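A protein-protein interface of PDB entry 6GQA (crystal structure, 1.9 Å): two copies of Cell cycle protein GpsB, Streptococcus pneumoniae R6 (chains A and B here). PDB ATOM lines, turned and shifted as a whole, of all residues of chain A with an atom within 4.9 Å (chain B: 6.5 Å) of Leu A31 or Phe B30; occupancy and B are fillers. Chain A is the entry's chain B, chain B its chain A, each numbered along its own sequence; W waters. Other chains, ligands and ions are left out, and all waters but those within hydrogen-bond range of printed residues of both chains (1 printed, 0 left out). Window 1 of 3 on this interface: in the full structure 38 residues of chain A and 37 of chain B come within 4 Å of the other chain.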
ATOM      1  N   PHE A   5      -9.972   7.956   2.807  1.00  0.00           N
ATOM      2  CA  PHE A   5     -10.870   7.711   1.682  1.00  0.00           C
ATOM      3  C   PHE A   5     -10.802   6.261   1.246  1.00  0.00           C
ATOM      4  O   PHE A   5      -9.734   5.673   1.260  1.00  0.00           O
ATOM      5  CB  PHE A   5     -10.473   8.565   0.485  1.00  0.00           C
ATOM      6  CG  PHE A   5     -10.745  10.038   0.690  1.00  0.00           C
ATOM      7  CD1 PHE A   5     -12.000  10.470   1.109  1.00  0.00           C
ATOM      8  CD2 PHE A   5      -9.741  10.963   0.500  1.00  0.00           C
ATOM      9  CE1 PHE A   5     -12.268  11.813   1.331  1.00  0.00           C
ATOM     10  CE2 PHE A   5      -9.994  12.344   0.704  1.00  0.00           C
ATOM     11  CZ  PHE A   5     -11.253  12.765   1.126  1.00  0.00           C
ATOM     12  N   ASP A   9     -15.117   6.342  -2.080  1.00  0.00           N
ATOM     13  CA  ASP A   9     -15.233   7.748  -1.716  1.00  0.00           C
ATOM     14  C   ASP A   9     -14.605   8.628  -2.782  1.00  0.00           C
ATOM     15  O   ASP A   9     -15.164   9.682  -3.130  1.00  0.00           O
ATOM     16  CB  ASP A   9     -14.554   8.042  -0.358  1.00  0.00           C
ATOM     17  CG  ASP A   9     -15.151   7.294   0.822  1.00  0.00           C
ATOM     18  OD1 ASP A   9     -16.364   6.977   0.869  1.00  0.00           O
ATOM     19  OD2 ASP A   9     -14.375   7.056   1.779  1.00  0.00           O
ATOM     20  N   ILE A  10     -13.413   8.242  -3.281  1.00  0.00           N
ATOM     21  CA  ILE A  10     -12.756   9.012  -4.354  1.00  0.00           C
ATOM     22  C   ILE A  10     -13.706   9.191  -5.521  1.00  0.00           C
ATOM     23  O   ILE A  10     -13.934  10.297  -6.014  1.00  0.00           O
ATOM     24  CB  ILE A  10     -11.471   8.333  -4.858  1.00  0.00           C
ATOM     25  CG1 ILE A  10     -10.423   8.171  -3.748  1.00  0.00           C
ATOM     26  CG2 ILE A  10     -10.909   9.166  -6.044  1.00  0.00           C
ATOM     27  CD1 ILE A  10     -10.354   9.312  -2.791  1.00  0.00           C
ATOM     28  N   GLN A  13     -16.900  11.518  -4.889  1.00  0.00           N
ATOM     29  CA  GLN A  13     -16.672  12.895  -4.499  1.00  0.00           C
ATOM     30  C   GLN A  13     -17.223  13.870  -5.524  1.00  0.00           C
ATOM     31  O   GLN A  13     -16.885  13.818  -6.709  1.00  0.00           O
ATOM     32  CB  GLN A  13     -15.181  13.158  -4.308  1.00  0.00           C
ATOM     33  CG  GLN A  13     -14.895  14.621  -3.866  1.00  0.00           C
ATOM     34  CD  GLN A  13     -15.329  14.943  -2.431  1.00  0.00           C
ATOM     35  OE1 GLN A  13     -15.188  14.127  -1.498  1.00  0.00           O
ATOM     36  NE2 GLN A  13     -15.827  16.150  -2.237  1.00  0.00           N
ATOM     37  N   PHE A  15     -17.812  17.963  -6.577  1.00  0.00           N
ATOM     38  CA  PHE A  15     -17.302  19.299  -6.292  1.00  0.00           C
ATOM     39  C   PHE A  15     -18.343  20.309  -6.742  1.00  0.00           C
ATOM     40  O   PHE A  15     -19.058  20.062  -7.715  1.00  0.00           O
ATOM     41  CB  PHE A  15     -15.975  19.566  -7.012  1.00  0.00           C
ATOM     42  CG  PHE A  15     -14.907  18.548  -6.669  1.00  0.00           C
ATOM     43  CD1 PHE A  15     -14.355  18.526  -5.382  1.00  0.00           C
ATOM     44  CD2 PHE A  15     -14.469  17.624  -7.612  1.00  0.00           C
ATOM     45  CE1 PHE A  15     -13.400  17.575  -4.993  1.00  0.00           C
ATOM     46  CE2 PHE A  15     -13.456  16.706  -7.272  1.00  0.00           C
ATOM     47  CZ  PHE A  15     -12.936  16.694  -5.925  1.00  0.00           C
ATOM     48  N   VAL A  27      -9.763  17.124 -13.960  1.00  0.00           N
ATOM     49  CA  VAL A  27      -9.911  16.601 -12.599  1.00  0.00           C
ATOM     50  C   VAL A  27     -10.486  15.209 -12.633  1.00  0.00           C
ATOM     51  O   VAL A  27     -10.018  14.314 -11.919  1.00  0.00           O
ATOM     52  CB  VAL A  27     -10.780  17.531 -11.736  1.00  0.00           C
ATOM     53  CG1 VAL A  27     -11.157  16.922 -10.346  1.00  0.00           C
ATOM     54  CG2 VAL A  27     -10.041  18.805 -11.533  1.00  0.00           C
ATOM     55  N   ASP A  28     -11.504  14.992 -13.477  1.00  0.00           N
ATOM     56  CA  ASP A  28     -12.149  13.691 -13.499  1.00  0.00           C
ATOM     57  C   ASP A  28     -11.183  12.615 -13.973  1.00  0.00           C
ATOM     58  O   ASP A  28     -11.086  11.539 -13.355  1.00  0.00           O
ATOM     59  CB  ASP A  28     -13.384  13.723 -14.386  1.00  0.00           C
ATOM     60  CG  ASP A  28     -14.572  14.553 -13.774  1.00  0.00           C
ATOM     61  OD1 ASP A  28     -14.582  14.911 -12.574  1.00  0.00           O
ATOM     62  OD2 ASP A  28     -15.550  14.778 -14.522  1.00  0.00           O
ATOM     63  N   GLU A  29     -10.453  12.887 -15.060  1.00  0.00           N
ATOM     64  CA  GLU A  29      -9.526  11.872 -15.576  1.00  0.00           C
ATOM     65  C   GLU A  29      -8.376  11.645 -14.609  1.00  0.00           C
ATOM     66  O   GLU A  29      -7.850  10.527 -14.476  1.00  0.00           O
ATOM     67  CB  GLU A  29      -9.005  12.320 -16.931  1.00  0.00           C
ATOM     68  CG  GLU A  29     -10.073  12.262 -18.011  1.00  0.00           C
ATOM     69  CD  GLU A  29      -9.500  12.473 -19.399  1.00  0.00           C
ATOM     70  OE1 GLU A  29      -8.405  13.091 -19.544  1.00  0.00           O
ATOM     71  OE2 GLU A  29     -10.152  12.019 -20.344  1.00  0.00           O
ATOM     72  N   PHE A  30      -8.001  12.688 -13.892  1.00  0.00           N
ATOM     73  CA  PHE A  30      -6.959  12.525 -12.880  1.00  0.00           C
ATOM     74  C   PHE A  30      -7.419  11.602 -11.768  1.00  0.00           C
ATOM     75  O   PHE A  30      -6.733  10.631 -11.451  1.00  0.00           O
ATOM     76  CB  PHE A  30      -6.571  13.879 -12.328  1.00  0.00           C
ATOM     77  CG  PHE A  30      -5.612  13.835 -11.203  1.00  0.00           C
ATOM     78  CD1 PHE A  30      -4.307  13.454 -11.402  1.00  0.00           C
ATOM     79  CD2 PHE A  30      -6.013  14.220  -9.931  1.00  0.00           C
ATOM     80  CE1 PHE A  30      -3.378  13.433 -10.271  1.00  0.00           C
ATOM     81  CE2 PHE A  30      -5.143  14.218  -8.880  1.00  0.00           C
ATOM     82  CZ  PHE A  30      -3.825  13.846  -9.048  1.00  0.00           C
ATOM     83  N   LEU A  31      -8.587  11.879 -11.183  1.00  0.00           N
ATOM     84  CA  LEU A  31      -9.139  11.050 -10.103  1.00  0.00           C
ATOM     85  C   LEU A  31      -9.458   9.637 -10.564  1.00  0.00           C
ATOM     86  O   LEU A  31      -9.447   8.691  -9.738  1.00  0.00           O
ATOM     87  CB  LEU A  31     -10.434  11.687  -9.554  1.00  0.00           C
ATOM     88  CG  LEU A  31     -10.167  13.021  -8.879  1.00  0.00           C
ATOM     89  CD1 LEU A  31     -11.506  13.573  -8.265  1.00  0.00           C
ATOM     90  CD2 LEU A  31      -9.039  12.820  -7.852  1.00  0.00           C
ATOM     91  N   ASP A  32      -9.783   9.465 -11.860  1.00  0.00           N
ATOM     92  CA  ASP A  32      -9.935   8.107 -12.402  1.00  0.00           C
ATOM     93  C   ASP A  32      -8.688   7.255 -12.127  1.00  0.00           C
ATOM     94  O   ASP A  32      -8.797   6.077 -11.753  1.00  0.00           O
ATOM     95  CB  ASP A  32     -10.212   8.172 -13.899  1.00  0.00           C
ATOM     96  CG  ASP A  32     -11.649   8.527 -14.210  1.00  0.00           C
ATOM     97  OD1 ASP A  32     -12.487   8.520 -13.267  1.00  0.00           O
ATOM     98  OD2 ASP A  32     -11.943   8.784 -15.416  1.00  0.00           O
ATOM     99  N   ASP A  33      -7.495   7.849 -12.316  1.00  0.00           N
ATOM    100  CA  ASP A  33      -6.224   7.150 -12.048  1.00  0.00           C
ATOM    101  C   ASP A  33      -5.973   7.044 -10.556  1.00  0.00           C
ATOM    102  O   ASP A  33      -5.429   6.030 -10.083  1.00  0.00           O
ATOM    103  CB  ASP A  33      -5.045   7.870 -12.714  1.00  0.00           C
ATOM    104  CG  ASP A  33      -4.867   7.491 -14.209  1.00  0.00           C
ATOM    105  OD1 ASP A  33      -5.385   6.457 -14.637  1.00  0.00           O
ATOM    106  OD2 ASP A  33      -4.204   8.207 -14.958  1.00  0.00           O
ATOM    107  N   VAL A  34      -6.307   8.095  -9.795  1.00  0.00           N
ATOM    108  CA  VAL A  34      -6.196   8.008  -8.336  1.00  0.00           C
ATOM    109  C   VAL A  34      -7.040   6.859  -7.800  1.00  0.00           C
ATOM    110  O   VAL A  34      -6.606   6.111  -6.924  1.00  0.00           O
ATOM    111  CB  VAL A  34      -6.579   9.355  -7.689  1.00  0.00           C
ATOM    112  CG1 VAL A  34      -6.837   9.207  -6.162  1.00  0.00           C
ATOM    113  CG2 VAL A  34      -5.510  10.388  -7.925  1.00  0.00           C
ATOM    114  N   ILE A  35      -8.221   6.643  -8.370  1.00  0.00           N
ATOM    115  CA  ILE A  35      -9.034   5.505  -7.966  1.00  0.00           C
ATOM    116  C   ILE A  35      -8.278   4.191  -8.124  1.00  0.00           C
ATOM    117  O   ILE A  35      -8.408   3.292  -7.281  1.00  0.00           O
ATOM    118  CB  ILE A  35     -10.335   5.484  -8.782  1.00  0.00           C
ATOM    119  CG1 ILE A  35     -11.304   6.534  -8.210  1.00  0.00           C
ATOM    120  CG2 ILE A  35     -10.941   4.088  -8.773  1.00  0.00           C
ATOM    121  CD1 ILE A  35     -12.375   7.028  -9.201  1.00  0.00           C
ATOM    122  N   PHE B   5       0.747   7.018  -9.293  1.00  0.00           N
ATOM    123  CA  PHE B   5       1.151   8.291  -8.723  1.00  0.00           C
ATOM    124  C   PHE B   5       1.935   8.068  -7.461  1.00  0.00           C
ATOM    125  O   PHE B   5       1.767   7.042  -6.821  1.00  0.00           O
ATOM    126  CB  PHE B   5      -0.064   9.117  -8.380  1.00  0.00           C
ATOM    127  CG  PHE B   5      -0.832   9.529  -9.572  1.00  0.00           C
ATOM    128  CD1 PHE B   5      -0.180  10.171 -10.627  1.00  0.00           C
ATOM    129  CD2 PHE B   5      -2.195   9.306  -9.642  1.00  0.00           C
ATOM    130  CE1 PHE B   5      -0.845  10.591 -11.741  1.00  0.00           C
ATOM    131  CE2 PHE B   5      -2.886   9.732 -10.797  1.00  0.00           C
ATOM    132  CZ  PHE B   5      -2.191  10.371 -11.843  1.00  0.00           C
ATOM    133  N   PHE B  15      -4.255  21.860 -13.090  1.00  0.00           N
ATOM    134  CA  PHE B  15      -5.455  21.731 -13.895  1.00  0.00           C
ATOM    135  C   PHE B  15      -5.708  23.031 -14.638  1.00  0.00           C
ATOM    136  O   PHE B  15      -5.456  24.101 -14.103  1.00  0.00           O
ATOM    137  CB  PHE B  15      -6.660  21.396 -12.996  1.00  0.00           C
ATOM    138  CG  PHE B  15      -6.471  20.156 -12.139  1.00  0.00           C
ATOM    139  CD1 PHE B  15      -6.499  18.915 -12.716  1.00  0.00           C
ATOM    140  CD2 PHE B  15      -6.320  20.252 -10.767  1.00  0.00           C
ATOM    141  CE1 PHE B  15      -6.345  17.777 -11.970  1.00  0.00           C
ATOM    142  CE2 PHE B  15      -6.191  19.106  -9.964  1.00  0.00           C
ATOM    143  CZ  PHE B  15      -6.192  17.849 -10.561  1.00  0.00           C
ATOM    144  N   TYR B  22     -14.914  23.196 -11.466  1.00  0.00           N
ATOM    145  CA  TYR B  22     -15.002  22.735 -10.088  1.00  0.00           C
ATOM    146  C   TYR B  22     -14.357  23.738  -9.123  1.00  0.00           C
ATOM    147  O   TYR B  22     -13.288  24.308  -9.399  1.00  0.00           O
ATOM    148  CB  TYR B  22     -14.298  21.372  -9.926  1.00  0.00           C
ATOM    149  CG  TYR B  22     -14.903  20.150 -10.569  1.00  0.00           C
ATOM    150  CD1 TYR B  22     -16.280  19.935 -10.592  1.00  0.00           C
ATOM    151  CD2 TYR B  22     -14.084  19.174 -11.118  1.00  0.00           C
ATOM    152  CE1 TYR B  22     -16.830  18.757 -11.187  1.00  0.00           C
ATOM    153  CE2 TYR B  22     -14.607  17.999 -11.708  1.00  0.00           C
ATOM    154  CZ  TYR B  22     -15.972  17.819 -11.739  1.00  0.00           C
ATOM    155  OH  TYR B  22     -16.433  16.669 -12.296  1.00  0.00           O
ATOM    156  N   VAL B  25     -10.886  25.365  -4.259  1.00  0.00           N
ATOM    157  CA  VAL B  25     -10.592  25.072  -2.857  1.00  0.00           C
ATOM    158  C   VAL B  25     -11.067  23.671  -2.490  1.00  0.00           C
ATOM    159  O   VAL B  25     -10.370  22.925  -1.795  1.00  0.00           O
ATOM    160  CB  VAL B  25     -11.239  26.112  -1.945  1.00  0.00           C
ATOM    161  CG1 VAL B  25     -11.058  25.651  -0.504  1.00  0.00           C
ATOM    162  CG2 VAL B  25     -10.595  27.457  -2.147  1.00  0.00           C
ATOM    163  N   GLU B  26     -12.292  23.318  -2.902  1.00  0.00           N
ATOM    164  CA  GLU B  26     -12.810  21.985  -2.602  1.00  0.00           C
ATOM    165  C   GLU B  26     -11.898  20.911  -3.169  1.00  0.00           C
ATOM    166  O   GLU B  26     -11.569  19.932  -2.469  1.00  0.00           O
ATOM    167  CB  GLU B  26     -14.235  21.821  -3.140  1.00  0.00           C
ATOM    168  CG  GLU B  26     -15.258  22.708  -2.436  1.00  0.00           C
ATOM    169  CD  GLU B  26     -16.688  22.553  -3.016  1.00  0.00           C
ATOM    170  OE1 GLU B  26     -16.985  21.535  -3.649  1.00  0.00           O
ATOM    171  OE2 GLU B  26     -17.517  23.453  -2.825  1.00  0.00           O
ATOM    172  N   VAL B  27     -11.459  21.080  -4.420  1.00  0.00           N
ATOM    173  CA  VAL B  27     -10.533  20.106  -5.029  1.00  0.00           C
ATOM    174  C   VAL B  27      -9.218  20.085  -4.259  1.00  0.00           C
ATOM    175  O   VAL B  27      -8.732  19.023  -3.858  1.00  0.00           O
ATOM    176  CB  VAL B  27     -10.296  20.415  -6.529  1.00  0.00           C
ATOM    177  CG1 VAL B  27      -9.212  19.552  -7.128  1.00  0.00           C
ATOM    178  CG2 VAL B  27     -11.604  20.195  -7.339  1.00  0.00           C
ATOM    179  N   ASP B  28      -8.604  21.252  -4.079  1.00  0.00           N
ATOM    180  CA  ASP B  28      -7.288  21.265  -3.443  1.00  0.00           C
ATOM    181  C   ASP B  28      -7.345  20.661  -2.054  1.00  0.00           C
ATOM    182  O   ASP B  28      -6.449  19.910  -1.647  1.00  0.00           O
ATOM    183  CB  ASP B  28      -6.778  22.679  -3.306  1.00  0.00           C
ATOM    184  CG  ASP B  28      -6.458  23.321  -4.589  1.00  0.00           C
ATOM    185  OD1 ASP B  28      -6.269  22.691  -5.651  1.00  0.00           O
ATOM    186  OD2 ASP B  28      -6.372  24.529  -4.492  1.00  0.00           O
ATOM    187  N   GLU B  29      -8.369  21.018  -1.300  1.00  0.00           N
ATOM    188  CA  GLU B  29      -8.557  20.478   0.040  1.00  0.00           C
ATOM    189  C   GLU B  29      -8.867  18.985   0.034  1.00  0.00           C
ATOM    190  O   GLU B  29      -8.469  18.256   0.962  1.00  0.00           O
ATOM    191  CB  GLU B  29      -9.652  21.265   0.726  1.00  0.00           C
ATOM    192  CG  GLU B  29      -9.104  22.563   1.336  1.00  0.00           C
ATOM    193  CD  GLU B  29     -10.146  23.307   2.180  1.00  0.00           C
ATOM    194  OE1 GLU B  29     -11.273  22.774   2.283  1.00  0.00           O
ATOM    195  OE2 GLU B  29      -9.837  24.410   2.718  1.00  0.00           O
ATOM    196  N   PHE B  30      -9.578  18.511  -0.981  1.00  0.00           N
ATOM    197  CA  PHE B  30      -9.694  17.066  -1.194  1.00  0.00           C
ATOM    198  C   PHE B  30      -8.326  16.423  -1.478  1.00  0.00           C
ATOM    199  O   PHE B  30      -7.952  15.394  -0.865  1.00  0.00           O
ATOM    200  CB  PHE B  30     -10.664  16.822  -2.354  1.00  0.00           C
ATOM    201  CG  PHE B  30     -10.892  15.370  -2.702  1.00  0.00           C
ATOM    202  CD1 PHE B  30     -11.676  14.550  -1.897  1.00  0.00           C
ATOM    203  CD2 PHE B  30     -10.373  14.837  -3.889  1.00  0.00           C
ATOM    204  CE1 PHE B  30     -11.883  13.202  -2.245  1.00  0.00           C
ATOM    205  CE2 PHE B  30     -10.639  13.534  -4.262  1.00  0.00           C
ATOM    206  CZ  PHE B  30     -11.389  12.707  -3.433  1.00  0.00           C
ATOM    207  N   LEU B  31      -7.554  17.003  -2.405  1.00  0.00           N
ATOM    208  CA  LEU B  31      -6.300  16.337  -2.757  1.00  0.00           C
ATOM    209  C   LEU B  31      -5.294  16.356  -1.602  1.00  0.00           C
ATOM    210  O   LEU B  31      -4.457  15.449  -1.486  1.00  0.00           O
ATOM    211  CB  LEU B  31      -5.682  16.967  -4.002  1.00  0.00           C
ATOM    212  CG  LEU B  31      -6.478  16.767  -5.321  1.00  0.00           C
ATOM    213  CD1 LEU B  31      -5.706  17.251  -6.549  1.00  0.00           C
ATOM    214  CD2 LEU B  31      -6.891  15.376  -5.485  1.00  0.00           C
ATOM    215  N   ASP B  32      -5.331  17.387  -0.759  1.00  0.00           N
ATOM    216  CA  ASP B  32      -4.493  17.361   0.432  1.00  0.00           C
ATOM    217  C   ASP B  32      -4.722  16.093   1.263  1.00  0.00           C
ATOM    218  O   ASP B  32      -3.770  15.532   1.801  1.00  0.00           O
ATOM    219  CB  ASP B  32      -4.734  18.602   1.257  1.00  0.00           C
ATOM    220  CG  ASP B  32      -4.076  19.826   0.631  1.00  0.00           C
ATOM    221  OD1 ASP B  32      -3.184  19.633  -0.223  1.00  0.00           O
ATOM    222  OD2 ASP B  32      -4.452  20.948   0.995  1.00  0.00           O
ATOM    223  N   ASP B  33      -5.969  15.610   1.367  1.00  0.00           N
ATOM    224  CA  ASP B  33      -6.166  14.389   2.135  1.00  0.00           C
ATOM    225  C   ASP B  33      -5.770  13.162   1.346  1.00  0.00           C
ATOM    226  O   ASP B  33      -5.233  12.222   1.929  1.00  0.00           O
ATOM    227  CB  ASP B  33      -7.600  14.257   2.634  1.00  0.00           C
ATOM    228  CG  ASP B  33      -7.879  15.124   3.871  1.00  0.00           C
ATOM    229  OD1 ASP B  33      -6.977  15.384   4.718  1.00  0.00           O
ATOM    230  OD2 ASP B  33      -9.026  15.537   4.026  1.00  0.00           O
ATOM    231  N   VAL B  34      -5.999  13.159   0.028  1.00  0.00           N
ATOM    232  CA  VAL B  34      -5.485  12.114  -0.867  1.00  0.00           C
ATOM    233  C   VAL B  34      -3.955  11.945  -0.719  1.00  0.00           C
ATOM    234  O   VAL B  34      -3.447  10.820  -0.658  1.00  0.00           O
ATOM    235  CB  VAL B  34      -5.884  12.446  -2.308  1.00  0.00           C
ATOM    236  CG1 VAL B  34      -5.060  11.659  -3.355  1.00  0.00           C
ATOM    237  CG2 VAL B  34      -7.380  12.226  -2.506  1.00  0.00           C
ATOM    238  N   ILE B  35      -3.212  13.051  -0.649  1.00  0.00           N
ATOM    239  CA  ILE B  35      -1.778  12.978  -0.367  1.00  0.00           C
ATOM    240  C   ILE B  35      -1.504  12.232   0.932  1.00  0.00           C
ATOM    241  O   ILE B  35      -0.542  11.453   1.021  1.00  0.00           O
ATOM    242  CB  ILE B  35      -1.201  14.396  -0.334  1.00  0.00           C
ATOM    243  CG1 ILE B  35      -1.130  14.951  -1.783  1.00  0.00           C
ATOM    244  CG2 ILE B  35       0.130  14.465   0.376  1.00  0.00           C
ATOM    245  CD1 ILE B  35      -1.234  16.469  -1.772  1.00  0.00           C
HETATM  246  O   HOH W   1     -16.667  15.560  -9.028  1.00  0.00           O
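Hydrophobic or aromatic side chains of chain B within 4 Å of the printed part of chain A: Phe B5, Phe B15, Tyr B22, Val B27, Phe B30 and Leu B31.
Along chain B the printed residues that touch a printed residue of chain A span positions 5 to 33.
Of the 14 printed residues of chain A, 10 touch a printed residue of chain B.
Among the printed residues, 17 pairs touch across the chains.
Among the printed residues, no Asp or Glu carboxylate lies within 4 Å of a Lys or Arg side-chain nitrogen of the other chain.
The side-chain hydroxyl of Tyr B22 sits at hydrogen-bond distance from the side-chain carboxylate of Asp A28, at 2.6 Å.
Phe A5 touches Phe B30, and with the chains exchanged Phe A30 touches Phe B5.
Phe A5 touches Asp B33, and with the chains exchanged Asp A33 touches Phe B5.
Phe A15 touches Phe B30, and with the chains exchanged Phe A30 touches Phe B15.
Val A34 touches Phe B5, but with the chains exchanged Phe A5 does not touch Val B34 (4.03 Å).
Positions printed for both chains: 5, 15, 27, 28, 29, 30, 31, 32, 33, 34 and 35.
Of the 17 pairs that touch across the chains among the printed residues, 10 have their exchanged pair printed and touching as well.
CB of Asp B33 touches CE2 of Phe A5, 3.6 Å away.
CD1 of Ile A10 touches CZ of Phe B30, 3.6 Å away.
Phe A15 touches Tyr B22 (CB to CD1, 3.6 Å).
Phe A15 touches Glu B26.
Phe A15 touches Val B27 (CG to CG2, 3.8 Å).
Phe A15 touches Phe B30 (CZ to CD2, 3.8 Å).
CG2 of Val A27 touches CD1 of Phe B15 (3.7 Å).
Phe A30 touches Phe B15 (CD2 to CZ, 3.7 Å).
CB of Asp A33 touches CE2 of Phe B5, at 3.4 Å.
CG2 of Val A34 touches CD2 of Phe B5, 3.9 Å away.
Of the printed residues of chain B, Ile A10 touches Phe B30.
Of the printed residues of chain B, Asp A28 touches Tyr B22.
Of the printed residues of chain B, Leu A31 touches Phe B30.
Val B25 touches none of the printed residues of chain A.
Glu B29 touches none of the printed residues of chain A.
Water W1 bridges the backbone carbonyl oxygen of Gln A13 (2.9 Å) and the side-chain hydroxyl of Tyr B22 (3.5 Å).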
